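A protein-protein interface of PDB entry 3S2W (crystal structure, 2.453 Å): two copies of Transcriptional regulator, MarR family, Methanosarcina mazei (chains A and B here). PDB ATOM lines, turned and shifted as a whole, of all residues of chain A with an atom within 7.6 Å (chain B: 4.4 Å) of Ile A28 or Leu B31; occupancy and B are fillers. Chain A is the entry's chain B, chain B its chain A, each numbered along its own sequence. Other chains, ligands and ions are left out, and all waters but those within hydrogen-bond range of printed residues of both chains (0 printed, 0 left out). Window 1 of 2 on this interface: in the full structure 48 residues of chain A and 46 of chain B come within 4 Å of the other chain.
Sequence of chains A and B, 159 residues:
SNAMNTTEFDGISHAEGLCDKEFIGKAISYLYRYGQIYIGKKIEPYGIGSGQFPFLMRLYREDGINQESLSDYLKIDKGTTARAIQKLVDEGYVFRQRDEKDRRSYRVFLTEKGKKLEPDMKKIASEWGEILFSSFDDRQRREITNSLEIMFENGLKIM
O of Leu B132 is in hydrogen-bond range of ND2 of Asn A154 (3.0 Å).
ND2 of Asn A154 lies within hydrogen-bond range of O of Ile A150.
Among the printed residues, merely in contact across the chains: Tyr A32 with Tyr B32 (3.1 Å), Met A151 with Leu B132 (3.4 Å), Met A151 with Leu B31 (3.5 Å), Phe A152 with Tyr B30 (3.5 Å), Ser A29 with Tyr B32 (3.6 Å), Ile A28 with Tyr B32 (3.6 Å), Leu A156 with Tyr B34 (3.7 Å), Phe A152 with Leu B31 (3.7 Å), Met A159 with Tyr B34 (3.7 Å), Ile A28 with Ile B28 (3.8 Å), Ile A28 with Leu B132 (3.8 Å), Tyr A32 with Ile B28 (3.8 Å), Tyr A32 with Ser B29 (3.8 Å), Gly A155 with Tyr B34 (3.9 Å), Arg A33 with Tyr B32 (3.9 Å), Phe A152 with Tyr B34 (3.9 Å), Leu A31 with Ile B28 (3.97 Å) and Ile A28 with Leu B31 (3.998 Å).
Of the printed residues of chain B, Ile A28 touches Ile B28 (3.8 Å), Leu B31 (3.998 Å), Tyr B32 (3.6 Å) and Leu B132 (3.8 Å). Printed residues of chain A within 4 Å of Leu B31: Ile A28, Met A151 and Phe A152. Of the printed residues of chain A, Tyr B30 touches Phe A152. Printed residues of chain B within 4 Å of Leu A31: Ile B28 (3.97 Å). Ser A147 touches none of the printed residues of chain B. The nearest printed residue of chain B that does not touch Ile A28 is Trp B128 (5.6 Å). The nearest printed residue of chain B that does not touch Phe A152 is Ala B27 (4.4 Å).
Of the 11 printed residues of chain B, 7 touch a printed residue of chain A. Hydrophobic or aromatic side chains of chain B that line the printed part of chain A: Ile B28, Tyr B30, Leu B31, Tyr B32, Tyr B34 and Leu B132. Printed residues of chain A that touch a printed residue of chain B: Ile A28, Ser A29, Leu A31, Tyr A32, Arg A33, Met A151, Phe A152, Asn A154, Gly A155, Leu A156 and Met A159. Among the printed residues, no Asp or Glu carboxylate lies within 4 Å of a Lys or Arg side-chain nitrogen of the other chain.
Ile A28 touches its own counterpart, Ile B28. Ile A28 touches Leu B31, and with the chains exchanged Leu A31 touches Ile B28. Ile A28 touches Tyr B32, and with the chains exchanged Tyr A32 touches Ile B28. Tyr B32 touches its own counterpart, Tyr A32. Positions printed for both chains: 27, 28, 29, 30, 31, 32, 33 and 34. Of the 19 pairs that touch across the chains among the printed residues, 8 have their exchanged pair printed and touching as well.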
ATOM      1  N   PHE A  23      -3.486  26.941 -13.736  1.00  0.00           N
ATOM      2  CA  PHE A  23      -2.383  27.861 -13.523  1.00  0.00           C
ATOM      3  C   PHE A  23      -1.047  27.147 -13.302  1.00  0.00           C
ATOM      4  O   PHE A  23       0.016  27.740 -13.458  1.00  0.00           O
ATOM      5  CB  PHE A  23      -2.683  28.786 -12.348  1.00  0.00           C
ATOM      6  CG  PHE A  23      -1.493  29.584 -11.898  1.00  0.00           C
ATOM      7  CD1 PHE A  23      -1.093  30.715 -12.602  1.00  0.00           C
ATOM      8  CD2 PHE A  23      -0.765  29.199 -10.778  1.00  0.00           C
ATOM      9  CE1 PHE A  23       0.016  31.454 -12.194  1.00  0.00           C
ATOM     10  CE2 PHE A  23       0.344  29.929 -10.354  1.00  0.00           C
ATOM     11  CZ  PHE A  23       0.737  31.059 -11.063  1.00  0.00           C
ATOM     12  N   ILE A  24      -1.089  25.875 -12.924  1.00  0.00           N
ATOM     13  CA  ILE A  24       0.160  25.176 -12.681  1.00  0.00           C
ATOM     14  C   ILE A  24       0.938  24.976 -13.999  1.00  0.00           C
ATOM     15  O   ILE A  24       2.151  25.152 -14.035  1.00  0.00           O
ATOM     16  CB  ILE A  24      -0.017  23.891 -11.833  1.00  0.00           C
ATOM     17  CG1 ILE A  24       1.281  23.608 -11.103  1.00  0.00           C
ATOM     18  CG2 ILE A  24      -0.524  22.715 -12.639  1.00  0.00           C
ATOM     19  CD1 ILE A  24       1.598  24.741 -10.158  1.00  0.00           C
ATOM     20  N   GLY A  25       0.232  24.676 -15.089  1.00  0.00           N
ATOM     21  CA  GLY A  25       0.849  24.720 -16.405  1.00  0.00           C
ATOM     22  C   GLY A  25       1.551  26.033 -16.760  1.00  0.00           C
ATOM     23  O   GLY A  25       2.706  26.052 -17.178  1.00  0.00           O
ATOM     24  N   LYS A  26       0.834  27.133 -16.607  1.00  0.00           N
ATOM     25  CA  LYS A  26       1.339  28.464 -16.887  1.00  0.00           C
ATOM     26  C   LYS A  26       2.551  28.805 -16.008  1.00  0.00           C
ATOM     27  O   LYS A  26       3.564  29.288 -16.505  1.00  0.00           O
ATOM     28  CB  LYS A  26       0.179  29.471 -16.708  1.00  0.00           C
ATOM     29  CG  LYS A  26       0.525  30.943 -16.582  1.00  0.00           C
ATOM     30  CD  LYS A  26      -0.761  31.777 -16.626  1.00  0.00           C
ATOM     31  CE  LYS A  26      -0.594  33.167 -15.985  1.00  0.00           C
ATOM     32  NZ  LYS A  26      -1.906  33.876 -15.720  1.00  0.00           N
ATOM     33  N   ALA A  27       2.470  28.528 -14.713  1.00  0.00           N
ATOM     34  CA  ALA A  27       3.607  28.799 -13.818  1.00  0.00           C
ATOM     35  C   ALA A  27       4.864  28.055 -14.281  1.00  0.00           C
ATOM     36  O   ALA A  27       5.946  28.640 -14.399  1.00  0.00           O
ATOM     37  CB  ALA A  27       3.260  28.444 -12.402  1.00  0.00           C
ATOM     38  N   ILE A  28       4.706  26.772 -14.603  1.00  0.00           N
ATOM     39  CA  ILE A  28       5.819  25.965 -15.097  1.00  0.00           C
ATOM     40  C   ILE A  28       6.422  26.477 -16.412  1.00  0.00           C
ATOM     41  O   ILE A  28       7.641  26.534 -16.560  1.00  0.00           O
ATOM     42  CB  ILE A  28       5.405  24.513 -15.236  1.00  0.00           C
ATOM     43  CG1 ILE A  28       5.202  23.929 -13.843  1.00  0.00           C
ATOM     44  CG2 ILE A  28       6.470  23.716 -15.983  1.00  0.00           C
ATOM     45  CD1 ILE A  28       4.365  22.730 -13.864  1.00  0.00           C
ATOM     46  N   SER A  29       5.559  26.839 -17.350  1.00  0.00           N
ATOM     47  CA  SER A  29       5.958  27.460 -18.616  1.00  0.00           C
ATOM     48  C   SER A  29       6.744  28.755 -18.462  1.00  0.00           C
ATOM     49  O   SER A  29       7.748  28.957 -19.135  1.00  0.00           O
ATOM     50  CB  SER A  29       4.724  27.772 -19.457  1.00  0.00           C
ATOM     51  OG  SER A  29       4.404  26.669 -20.268  1.00  0.00           O
ATOM     52  N   TYR A  30       6.251  29.651 -17.616  1.00  0.00           N
ATOM     53  CA  TYR A  30       6.976  30.890 -17.355  1.00  0.00           C
ATOM     54  C   TYR A  30       8.342  30.645 -16.686  1.00  0.00           C
ATOM     55  O   TYR A  30       9.352  31.161 -17.158  1.00  0.00           O
ATOM     56  CB  TYR A  30       6.120  31.870 -16.546  1.00  0.00           C
ATOM     57  CG  TYR A  30       5.116  32.635 -17.391  1.00  0.00           C
ATOM     58  CD1 TYR A  30       5.408  33.909 -17.878  1.00  0.00           C
ATOM     59  CD2 TYR A  30       3.887  32.079 -17.703  1.00  0.00           C
ATOM     60  CE1 TYR A  30       4.495  34.598 -18.640  1.00  0.00           C
ATOM     61  CE2 TYR A  30       2.972  32.750 -18.453  1.00  0.00           C
ATOM     62  CZ  TYR A  30       3.269  34.009 -18.925  1.00  0.00           C
ATOM     63  OH  TYR A  30       2.325  34.667 -19.686  1.00  0.00           O
ATOM     64  N   LEU A  31       8.380  29.848 -15.614  1.00  0.00           N
ATOM     65  CA  LEU A  31       9.660  29.458 -15.012  1.00  0.00           C
ATOM     66  C   LEU A  31      10.625  28.860 -16.032  1.00  0.00           C
ATOM     67  O   LEU A  31      11.814  29.171 -16.019  1.00  0.00           O
ATOM     68  CB  LEU A  31       9.454  28.494 -13.854  1.00  0.00           C
ATOM     69  CG  LEU A  31       8.786  29.161 -12.661  1.00  0.00           C
ATOM     70  CD1 LEU A  31       8.347  28.124 -11.626  1.00  0.00           C
ATOM     71  CD2 LEU A  31       9.727  30.196 -12.072  1.00  0.00           C
ATOM     72  N   TYR A  32      10.115  28.030 -16.937  1.00  0.00           N
ATOM     73  CA  TYR A  32      10.978  27.423 -17.949  1.00  0.00           C
ATOM     74  C   TYR A  32      11.592  28.508 -18.831  1.00  0.00           C
ATOM     75  O   TYR A  32      12.816  28.594 -18.970  1.00  0.00           O
ATOM     76  CB  TYR A  32      10.224  26.384 -18.807  1.00  0.00           C
ATOM     77  CG  TYR A  32      11.019  25.960 -20.020  1.00  0.00           C
ATOM     78  CD1 TYR A  32      10.702  26.438 -21.291  1.00  0.00           C
ATOM     79  CD2 TYR A  32      12.113  25.107 -19.896  1.00  0.00           C
ATOM     80  CE1 TYR A  32      11.440  26.067 -22.412  1.00  0.00           C
ATOM     81  CE2 TYR A  32      12.866  24.727 -21.011  1.00  0.00           C
ATOM     82  CZ  TYR A  32      12.520  25.208 -22.265  1.00  0.00           C
ATOM     83  OH  TYR A  32      13.252  24.846 -23.375  1.00  0.00           O
ATOM     84  N   ARG A  33      10.736  29.350 -19.403  1.00  0.00           N
ATOM     85  CA  ARG A  33      11.198  30.370 -20.329  1.00  0.00           C
ATOM     86  C   ARG A  33      12.095  31.381 -19.646  1.00  0.00           C
ATOM     87  O   ARG A  33      13.043  31.879 -20.237  1.00  0.00           O
ATOM     88  CB  ARG A  33      10.028  31.035 -21.052  1.00  0.00           C
ATOM     89  CG  ARG A  33       9.367  30.067 -22.056  1.00  0.00           C
ATOM     90  CD  ARG A  33       8.270  30.724 -22.877  1.00  0.00           C
ATOM     91  NE  ARG A  33       7.053  30.934 -22.095  1.00  0.00           N
ATOM     92  CZ  ARG A  33       5.994  30.127 -22.126  1.00  0.00           C
ATOM     93  NH1 ARG A  33       5.983  29.053 -22.913  1.00  0.00           N
ATOM     94  NH2 ARG A  33       4.936  30.401 -21.371  1.00  0.00           N
ATOM     95  N   TYR A  34      11.831  31.649 -18.381  1.00  0.00           N
ATOM     96  CA  TYR A  34      12.704  32.565 -17.647  1.00  0.00           C
ATOM     97  C   TYR A  34      14.068  31.923 -17.396  1.00  0.00           C
ATOM     98  O   TYR A  34      15.094  32.575 -17.553  1.00  0.00           O
ATOM     99  CB  TYR A  34      12.013  33.121 -16.386  1.00  0.00           C
ATOM    100  CG  TYR A  34      11.044  34.252 -16.750  1.00  0.00           C
ATOM    101  CD1 TYR A  34      10.018  34.041 -17.665  1.00  0.00           C
ATOM    102  CD2 TYR A  34      11.180  35.529 -16.219  1.00  0.00           C
ATOM    103  CE1 TYR A  34       9.151  35.046 -18.022  1.00  0.00           C
ATOM    104  CE2 TYR A  34      10.300  36.555 -16.572  1.00  0.00           C
ATOM    105  CZ  TYR A  34       9.287  36.304 -17.478  1.00  0.00           C
ATOM    106  OH  TYR A  34       8.408  37.307 -17.859  1.00  0.00           O
ATOM    107  N   SER A 147       7.292  17.905  -3.696  1.00  0.00           N
ATOM    108  CA  SER A 147       6.144  18.070  -4.571  1.00  0.00           C
ATOM    109  C   SER A 147       6.529  17.999  -6.055  1.00  0.00           C
ATOM    110  O   SER A 147       5.870  17.298  -6.842  1.00  0.00           O
ATOM    111  CB  SER A 147       5.422  19.379  -4.250  1.00  0.00           C
ATOM    112  OG  SER A 147       4.931  19.353  -2.919  1.00  0.00           O
ATOM    113  N   LEU A 148       7.593  18.709  -6.432  1.00  0.00           N
ATOM    114  CA  LEU A 148       8.079  18.663  -7.816  1.00  0.00           C
ATOM    115  C   LEU A 148       8.416  17.251  -8.282  1.00  0.00           C
ATOM    116  O   LEU A 148       8.084  16.895  -9.391  1.00  0.00           O
ATOM    117  CB  LEU A 148       9.292  19.562  -8.011  1.00  0.00           C
ATOM    118  CG  LEU A 148       8.988  21.052  -8.002  1.00  0.00           C
ATOM    119  CD1 LEU A 148      10.295  21.841  -8.059  1.00  0.00           C
ATOM    120  CD2 LEU A 148       8.057  21.404  -9.152  1.00  0.00           C
ATOM    121  N   GLU A 149       9.088  16.467  -7.436  1.00  0.00           N
ATOM    122  CA  GLU A 149       9.389  15.080  -7.753  1.00  0.00           C
ATOM    123  C   GLU A 149       8.108  14.313  -8.047  1.00  0.00           C
ATOM    124  O   GLU A 149       8.039  13.552  -9.004  1.00  0.00           O
ATOM    125  CB  GLU A 149      10.131  14.393  -6.603  1.00  0.00           C
ATOM    126  CG  GLU A 149      11.586  14.816  -6.465  1.00  0.00           C
ATOM    127  CD  GLU A 149      12.323  14.120  -5.311  1.00  0.00           C
ATOM    128  OE1 GLU A 149      13.351  14.661  -4.845  1.00  0.00           O
ATOM    129  OE2 GLU A 149      11.886  13.032  -4.873  1.00  0.00           O
ATOM    130  N   ILE A 150       7.098  14.500  -7.208  1.00  0.00           N
ATOM    131  CA  ILE A 150       5.838  13.803  -7.403  1.00  0.00           C
ATOM    132  C   ILE A 150       5.212  14.245  -8.714  1.00  0.00           C
ATOM    133  O   ILE A 150       4.782  13.419  -9.518  1.00  0.00           O
ATOM    134  CB  ILE A 150       4.876  14.004  -6.215  1.00  0.00           C
ATOM    135  CG1 ILE A 150       5.423  13.291  -4.968  1.00  0.00           C
ATOM    136  CG2 ILE A 150       3.499  13.459  -6.540  1.00  0.00           C
ATOM    137  CD1 ILE A 150       4.595  13.541  -3.693  1.00  0.00           C
ATOM    138  N   MET A 151       5.198  15.547  -8.957  1.00  0.00           N
ATOM    139  CA  MET A 151       4.609  16.044 -10.190  1.00  0.00           C
ATOM    140  C   MET A 151       5.379  15.534 -11.387  1.00  0.00           C
ATOM    141  O   MET A 151       4.793  15.095 -12.381  1.00  0.00           O
ATOM    142  CB  MET A 151       4.572  17.564 -10.193  1.00  0.00           C
ATOM    143  CG  MET A 151       3.610  18.108  -9.165  1.00  0.00           C
ATOM    144  SD  MET A 151       3.428  20.048  -9.232  1.00  0.00           S
ATOM    145  CE  MET A 151       2.214  20.223  -7.727  1.00  0.00           C
ATOM    146  N   PHE A 152       6.700  15.592 -11.279  1.00  0.00           N
ATOM    147  CA  PHE A 152       7.581  15.095 -12.323  1.00  0.00           C
ATOM    148  C   PHE A 152       7.229  13.661 -12.717  1.00  0.00           C
ATOM    149  O   PHE A 152       7.108  13.356 -13.892  1.00  0.00           O
ATOM    150  CB  PHE A 152       9.043  15.190 -11.882  1.00  0.00           C
ATOM    151  CG  PHE A 152       9.986  14.495 -12.805  1.00  0.00           C
ATOM    152  CD1 PHE A 152      10.348  13.171 -12.581  1.00  0.00           C
ATOM    153  CD2 PHE A 152      10.494  15.147 -13.913  1.00  0.00           C
ATOM    154  CE1 PHE A 152      11.220  12.514 -13.437  1.00  0.00           C
ATOM    155  CE2 PHE A 152      11.364  14.502 -14.774  1.00  0.00           C
ATOM    156  CZ  PHE A 152      11.727  13.183 -14.538  1.00  0.00           C
ATOM    157  N   GLU A 153       7.047  12.797 -11.727  1.00  0.00           N
ATOM    158  CA  GLU A 153       6.702  11.398 -11.969  1.00  0.00           C
ATOM    159  C   GLU A 153       5.285  11.229 -12.503  1.00  0.00           C
ATOM    160  O   GLU A 153       5.036  10.352 -13.321  1.00  0.00           O
ATOM    161  CB  GLU A 153       6.871  10.568 -10.689  1.00  0.00           C
ATOM    162  CG  GLU A 153       8.316  10.377 -10.227  1.00  0.00           C
ATOM    163  CD  GLU A 153       8.408   9.936  -8.769  1.00  0.00           C
ATOM    164  OE1 GLU A 153       9.511  10.001  -8.190  1.00  0.00           O
ATOM    165  OE2 GLU A 153       7.374   9.533  -8.194  1.00  0.00           O
ATOM    166  N   ASN A 154       4.355  12.049 -12.021  1.00  0.00           N
ATOM    167  CA  ASN A 154       2.983  11.998 -12.506  1.00  0.00           C
ATOM    168  C   ASN A 154       2.945  12.224 -14.005  1.00  0.00           C
ATOM    169  O   ASN A 154       2.301  11.472 -14.731  1.00  0.00           O
ATOM    170  CB  ASN A 154       2.115  13.042 -11.802  1.00  0.00           C
ATOM    171  CG  ASN A 154       1.658  12.594 -10.438  1.00  0.00           C
ATOM    172  OD1 ASN A 154       1.448  11.412 -10.211  1.00  0.00           O
ATOM    173  ND2 ASN A 154       1.491  13.537  -9.525  1.00  0.00           N
ATOM    174  N   GLY A 155       3.652  13.255 -14.463  1.00  0.00           N
ATOM    175  CA  GLY A 155       3.679  13.602 -15.873  1.00  0.00           C
ATOM    176  C   GLY A 155       4.497  12.648 -16.730  1.00  0.00           C
ATOM    177  O   GLY A 155       4.231  12.478 -17.930  1.00  0.00           O
ATOM    178  N   LEU A 156       5.495  12.024 -16.116  1.00  0.00           N
ATOM    179  CA  LEU A 156       6.306  11.040 -16.816  1.00  0.00           C
ATOM    180  C   LEU A 156       5.490   9.807 -17.166  1.00  0.00           C
ATOM    181  O   LEU A 156       5.692   9.201 -18.210  1.00  0.00           O
ATOM    182  CB  LEU A 156       7.524  10.641 -15.979  1.00  0.00           C
ATOM    183  CG  LEU A 156       8.338   9.461 -16.522  1.00  0.00           C
ATOM    184  CD1 LEU A 156       8.822   9.723 -17.964  1.00  0.00           C
ATOM    185  CD2 LEU A 156       9.509   9.108 -15.597  1.00  0.00           C
ATOM    186  N   MET A 159       3.447  10.006 -20.470  1.00  0.00           N
ATOM    187  CA  MET A 159       4.184   9.942 -21.726  1.00  0.00           C
ATOM    188  C   MET A 159       4.180   8.527 -22.280  1.00  0.00           C
ATOM    189  O   MET A 159       4.296   8.331 -23.487  1.00  0.00           O
ATOM    190  CB  MET A 159       5.619  10.399 -21.523  1.00  0.00           C
ATOM    191  CG  MET A 159       5.745  11.805 -21.000  1.00  0.00           C
ATOM    192  SD  MET A 159       5.410  13.170 -22.350  1.00  0.00           S
ATOM    193  CE  MET A 159       3.484  13.447 -22.106  1.00  0.00           C
ATOM    194  N   ALA B  27      13.559  19.522 -13.042  1.00  0.00           N
ATOM    195  CA  ALA B  27      12.163  19.115 -12.921  1.00  0.00           C
ATOM    196  C   ALA B  27      11.263  20.022 -13.782  1.00  0.00           C
ATOM    197  O   ALA B  27      10.356  19.560 -14.479  1.00  0.00           O
ATOM    198  CB  ALA B  27      11.719  19.118 -11.436  1.00  0.00           C
ATOM    199  N   ILE B  28      11.540  21.317 -13.727  1.00  0.00           N
ATOM    200  CA  ILE B  28      10.773  22.329 -14.440  1.00  0.00           C
ATOM    201  C   ILE B  28      10.878  22.186 -15.955  1.00  0.00           C
ATOM    202  O   ILE B  28       9.856  22.121 -16.643  1.00  0.00           O
ATOM    203  CB  ILE B  28      11.191  23.731 -13.958  1.00  0.00           C
ATOM    204  CG1 ILE B  28      10.670  23.921 -12.526  1.00  0.00           C
ATOM    205  CG2 ILE B  28      10.718  24.836 -14.911  1.00  0.00           C
ATOM    206  CD1 ILE B  28      11.052  25.227 -11.898  1.00  0.00           C
ATOM    207  N   SER B  29      12.099  22.095 -16.473  1.00  0.00           N
ATOM    208  CA  SER B  29      12.322  21.823 -17.898  1.00  0.00           C
ATOM    209  C   SER B  29      11.581  20.585 -18.396  1.00  0.00           C
ATOM    210  O   SER B  29      11.056  20.582 -19.493  1.00  0.00           O
ATOM    211  CB  SER B  29      13.806  21.612 -18.161  1.00  0.00           C
ATOM    212  OG  SER B  29      14.556  22.587 -17.466  1.00  0.00           O
ATOM    213  N   TYR B  30      11.560  19.523 -17.597  1.00  0.00           N
ATOM    214  CA  TYR B  30      10.863  18.314 -18.007  1.00  0.00           C
ATOM    215  C   TYR B  30       9.349  18.446 -17.988  1.00  0.00           C
ATOM    216  O   TYR B  30       8.668  17.977 -18.906  1.00  0.00           O
ATOM    217  CB  TYR B  30      11.289  17.117 -17.148  1.00  0.00           C
ATOM    218  CG  TYR B  30      12.587  16.484 -17.602  1.00  0.00           C
ATOM    219  CD1 TYR B  30      12.588  15.487 -18.569  1.00  0.00           C
ATOM    220  CD2 TYR B  30      13.813  16.892 -17.072  1.00  0.00           C
ATOM    221  CE1 TYR B  30      13.771  14.902 -18.997  1.00  0.00           C
ATOM    222  CE2 TYR B  30      15.001  16.319 -17.492  1.00  0.00           C
ATOM    223  CZ  TYR B  30      14.971  15.321 -18.457  1.00  0.00           C
ATOM    224  OH  TYR B  30      16.140  14.742 -18.890  1.00  0.00           O
ATOM    225  N   LEU B  31       8.816  19.068 -16.940  1.00  0.00           N
ATOM    226  CA  LEU B  31       7.377  19.204 -16.843  1.00  0.00           C
ATOM    227  C   LEU B  31       6.905  20.071 -18.002  1.00  0.00           C
ATOM    228  O   LEU B  31       5.914  19.761 -18.680  1.00  0.00           O
ATOM    229  CB  LEU B  31       6.980  19.781 -15.494  1.00  0.00           C
ATOM    230  CG  LEU B  31       7.130  18.817 -14.314  1.00  0.00           C
ATOM    231  CD1 LEU B  31       7.102  19.569 -13.010  1.00  0.00           C
ATOM    232  CD2 LEU B  31       6.063  17.750 -14.331  1.00  0.00           C
ATOM    233  N   TYR B  32       7.654  21.127 -18.264  1.00  0.00           N
ATOM    234  CA  TYR B  32       7.399  21.944 -19.438  1.00  0.00           C
ATOM    235  C   TYR B  32       7.322  21.124 -20.729  1.00  0.00           C
ATOM    236  O   TYR B  32       6.385  21.268 -21.515  1.00  0.00           O
ATOM    237  CB  TYR B  32       8.463  23.020 -19.591  1.00  0.00           C
ATOM    238  CG  TYR B  32       8.344  23.743 -20.908  1.00  0.00           C
ATOM    239  CD1 TYR B  32       7.352  24.706 -21.109  1.00  0.00           C
ATOM    240  CD2 TYR B  32       9.215  23.467 -21.954  1.00  0.00           C
ATOM    241  CE1 TYR B  32       7.233  25.382 -22.325  1.00  0.00           C
ATOM    242  CE2 TYR B  32       9.098  24.117 -23.161  1.00  0.00           C
ATOM    243  CZ  TYR B  32       8.107  25.084 -23.345  1.00  0.00           C
ATOM    244  OH  TYR B  32       8.002  25.738 -24.555  1.00  0.00           O
ATOM    245  N   ARG B  33       8.312  20.270 -20.958  1.00  0.00           N
ATOM    246  CA  ARG B  33       8.357  19.523 -22.215  1.00  0.00           C
ATOM    247  C   ARG B  33       7.278  18.478 -22.294  1.00  0.00           C
ATOM    248  O   ARG B  33       6.694  18.278 -23.355  1.00  0.00           O
ATOM    249  CB  ARG B  33       9.723  18.896 -22.447  1.00  0.00           C
ATOM    250  CG  ARG B  33      10.775  19.952 -22.666  1.00  0.00           C
ATOM    251  CD  ARG B  33      12.091  19.369 -23.137  1.00  0.00           C
ATOM    252  NE  ARG B  33      13.169  20.270 -22.763  1.00  0.00           N
ATOM    253  CZ  ARG B  33      14.045  20.029 -21.799  1.00  0.00           C
ATOM    254  NH1 ARG B  33      14.972  20.937 -21.530  1.00  0.00           N
ATOM    255  NH2 ARG B  33      14.004  18.879 -21.122  1.00  0.00           N
ATOM    256  N   TYR B  34       7.031  17.801 -21.176  1.00  0.00           N
ATOM    257  CA  TYR B  34       5.948  16.827 -21.104  1.00  0.00           C
ATOM    258  C   TYR B  34       4.647  17.562 -21.391  1.00  0.00           C
ATOM    259  O   TYR B  34       3.812  17.108 -22.184  1.00  0.00           O
ATOM    260  CB  TYR B  34       5.881  16.186 -19.712  1.00  0.00           C
ATOM    261  CG  TYR B  34       7.087  15.347 -19.342  1.00  0.00           C
ATOM    262  CD1 TYR B  34       7.992  14.923 -20.309  1.00  0.00           C
ATOM    263  CD2 TYR B  34       7.311  14.970 -18.028  1.00  0.00           C
ATOM    264  CE1 TYR B  34       9.079  14.164 -19.978  1.00  0.00           C
ATOM    265  CE2 TYR B  34       8.398  14.202 -17.682  1.00  0.00           C
ATOM    266  CZ  TYR B  34       9.283  13.799 -18.654  1.00  0.00           C
ATOM    267  OH  TYR B  34      10.368  13.018 -18.296  1.00  0.00           O
ATOM    268  N   GLY B  35       4.491  18.705 -20.726  1.00  0.00           N
ATOM    269  CA  GLY B  35       3.335  19.548 -20.916  1.00  0.00           C
ATOM    270  C   GLY B  35       3.111  19.845 -22.386  1.00  0.00           C
ATOM    271  O   GLY B  35       1.973  19.790 -22.848  1.00  0.00           O
ATOM    272  N   TRP B 128      -4.398  18.740 -17.735  1.00  0.00           N
ATOM    273  CA  TRP B 128      -2.975  18.637 -17.540  1.00  0.00           C
ATOM    274  C   TRP B 128      -2.597  18.885 -16.070  1.00  0.00           C
ATOM    275  O   TRP B 128      -1.844  18.103 -15.482  1.00  0.00           O
ATOM    276  CB  TRP B 128      -2.263  19.592 -18.475  1.00  0.00           C
ATOM    277  CG  TRP B 128      -0.807  19.605 -18.254  1.00  0.00           C
ATOM    278  CD1 TRP B 128      -0.046  20.675 -17.928  1.00  0.00           C
ATOM    279  CD2 TRP B 128       0.069  18.478 -18.280  1.00  0.00           C
ATOM    280  NE1 TRP B 128       1.262  20.298 -17.778  1.00  0.00           N
ATOM    281  CE2 TRP B 128       1.359  18.947 -17.977  1.00  0.00           C
ATOM    282  CE3 TRP B 128      -0.109  17.113 -18.544  1.00  0.00           C
ATOM    283  CZ2 TRP B 128       2.478  18.110 -17.950  1.00  0.00           C
ATOM    284  CZ3 TRP B 128       0.999  16.279 -18.498  1.00  0.00           C
ATOM    285  CH2 TRP B 128       2.279  16.790 -18.220  1.00  0.00           C
ATOM    286  N   LEU B 132      -1.018  16.523 -13.113  1.00  0.00           N
ATOM    287  CA  LEU B 132       0.152  16.836 -12.303  1.00  0.00           C
ATOM    288  C   LEU B 132      -0.120  16.718 -10.800  1.00  0.00           C
ATOM    289  O   LEU B 132       0.776  16.368 -10.026  1.00  0.00           O
ATOM    290  CB  LEU B 132       0.715  18.214 -12.644  1.00  0.00           C
ATOM    291  CG  LEU B 132       1.306  18.403 -14.043  1.00  0.00           C
ATOM    292  CD1 LEU B 132       1.922  19.813 -14.227  1.00  0.00           C
ATOM    293  CD2 LEU B 132       2.342  17.326 -14.315  1.00  0.00           C
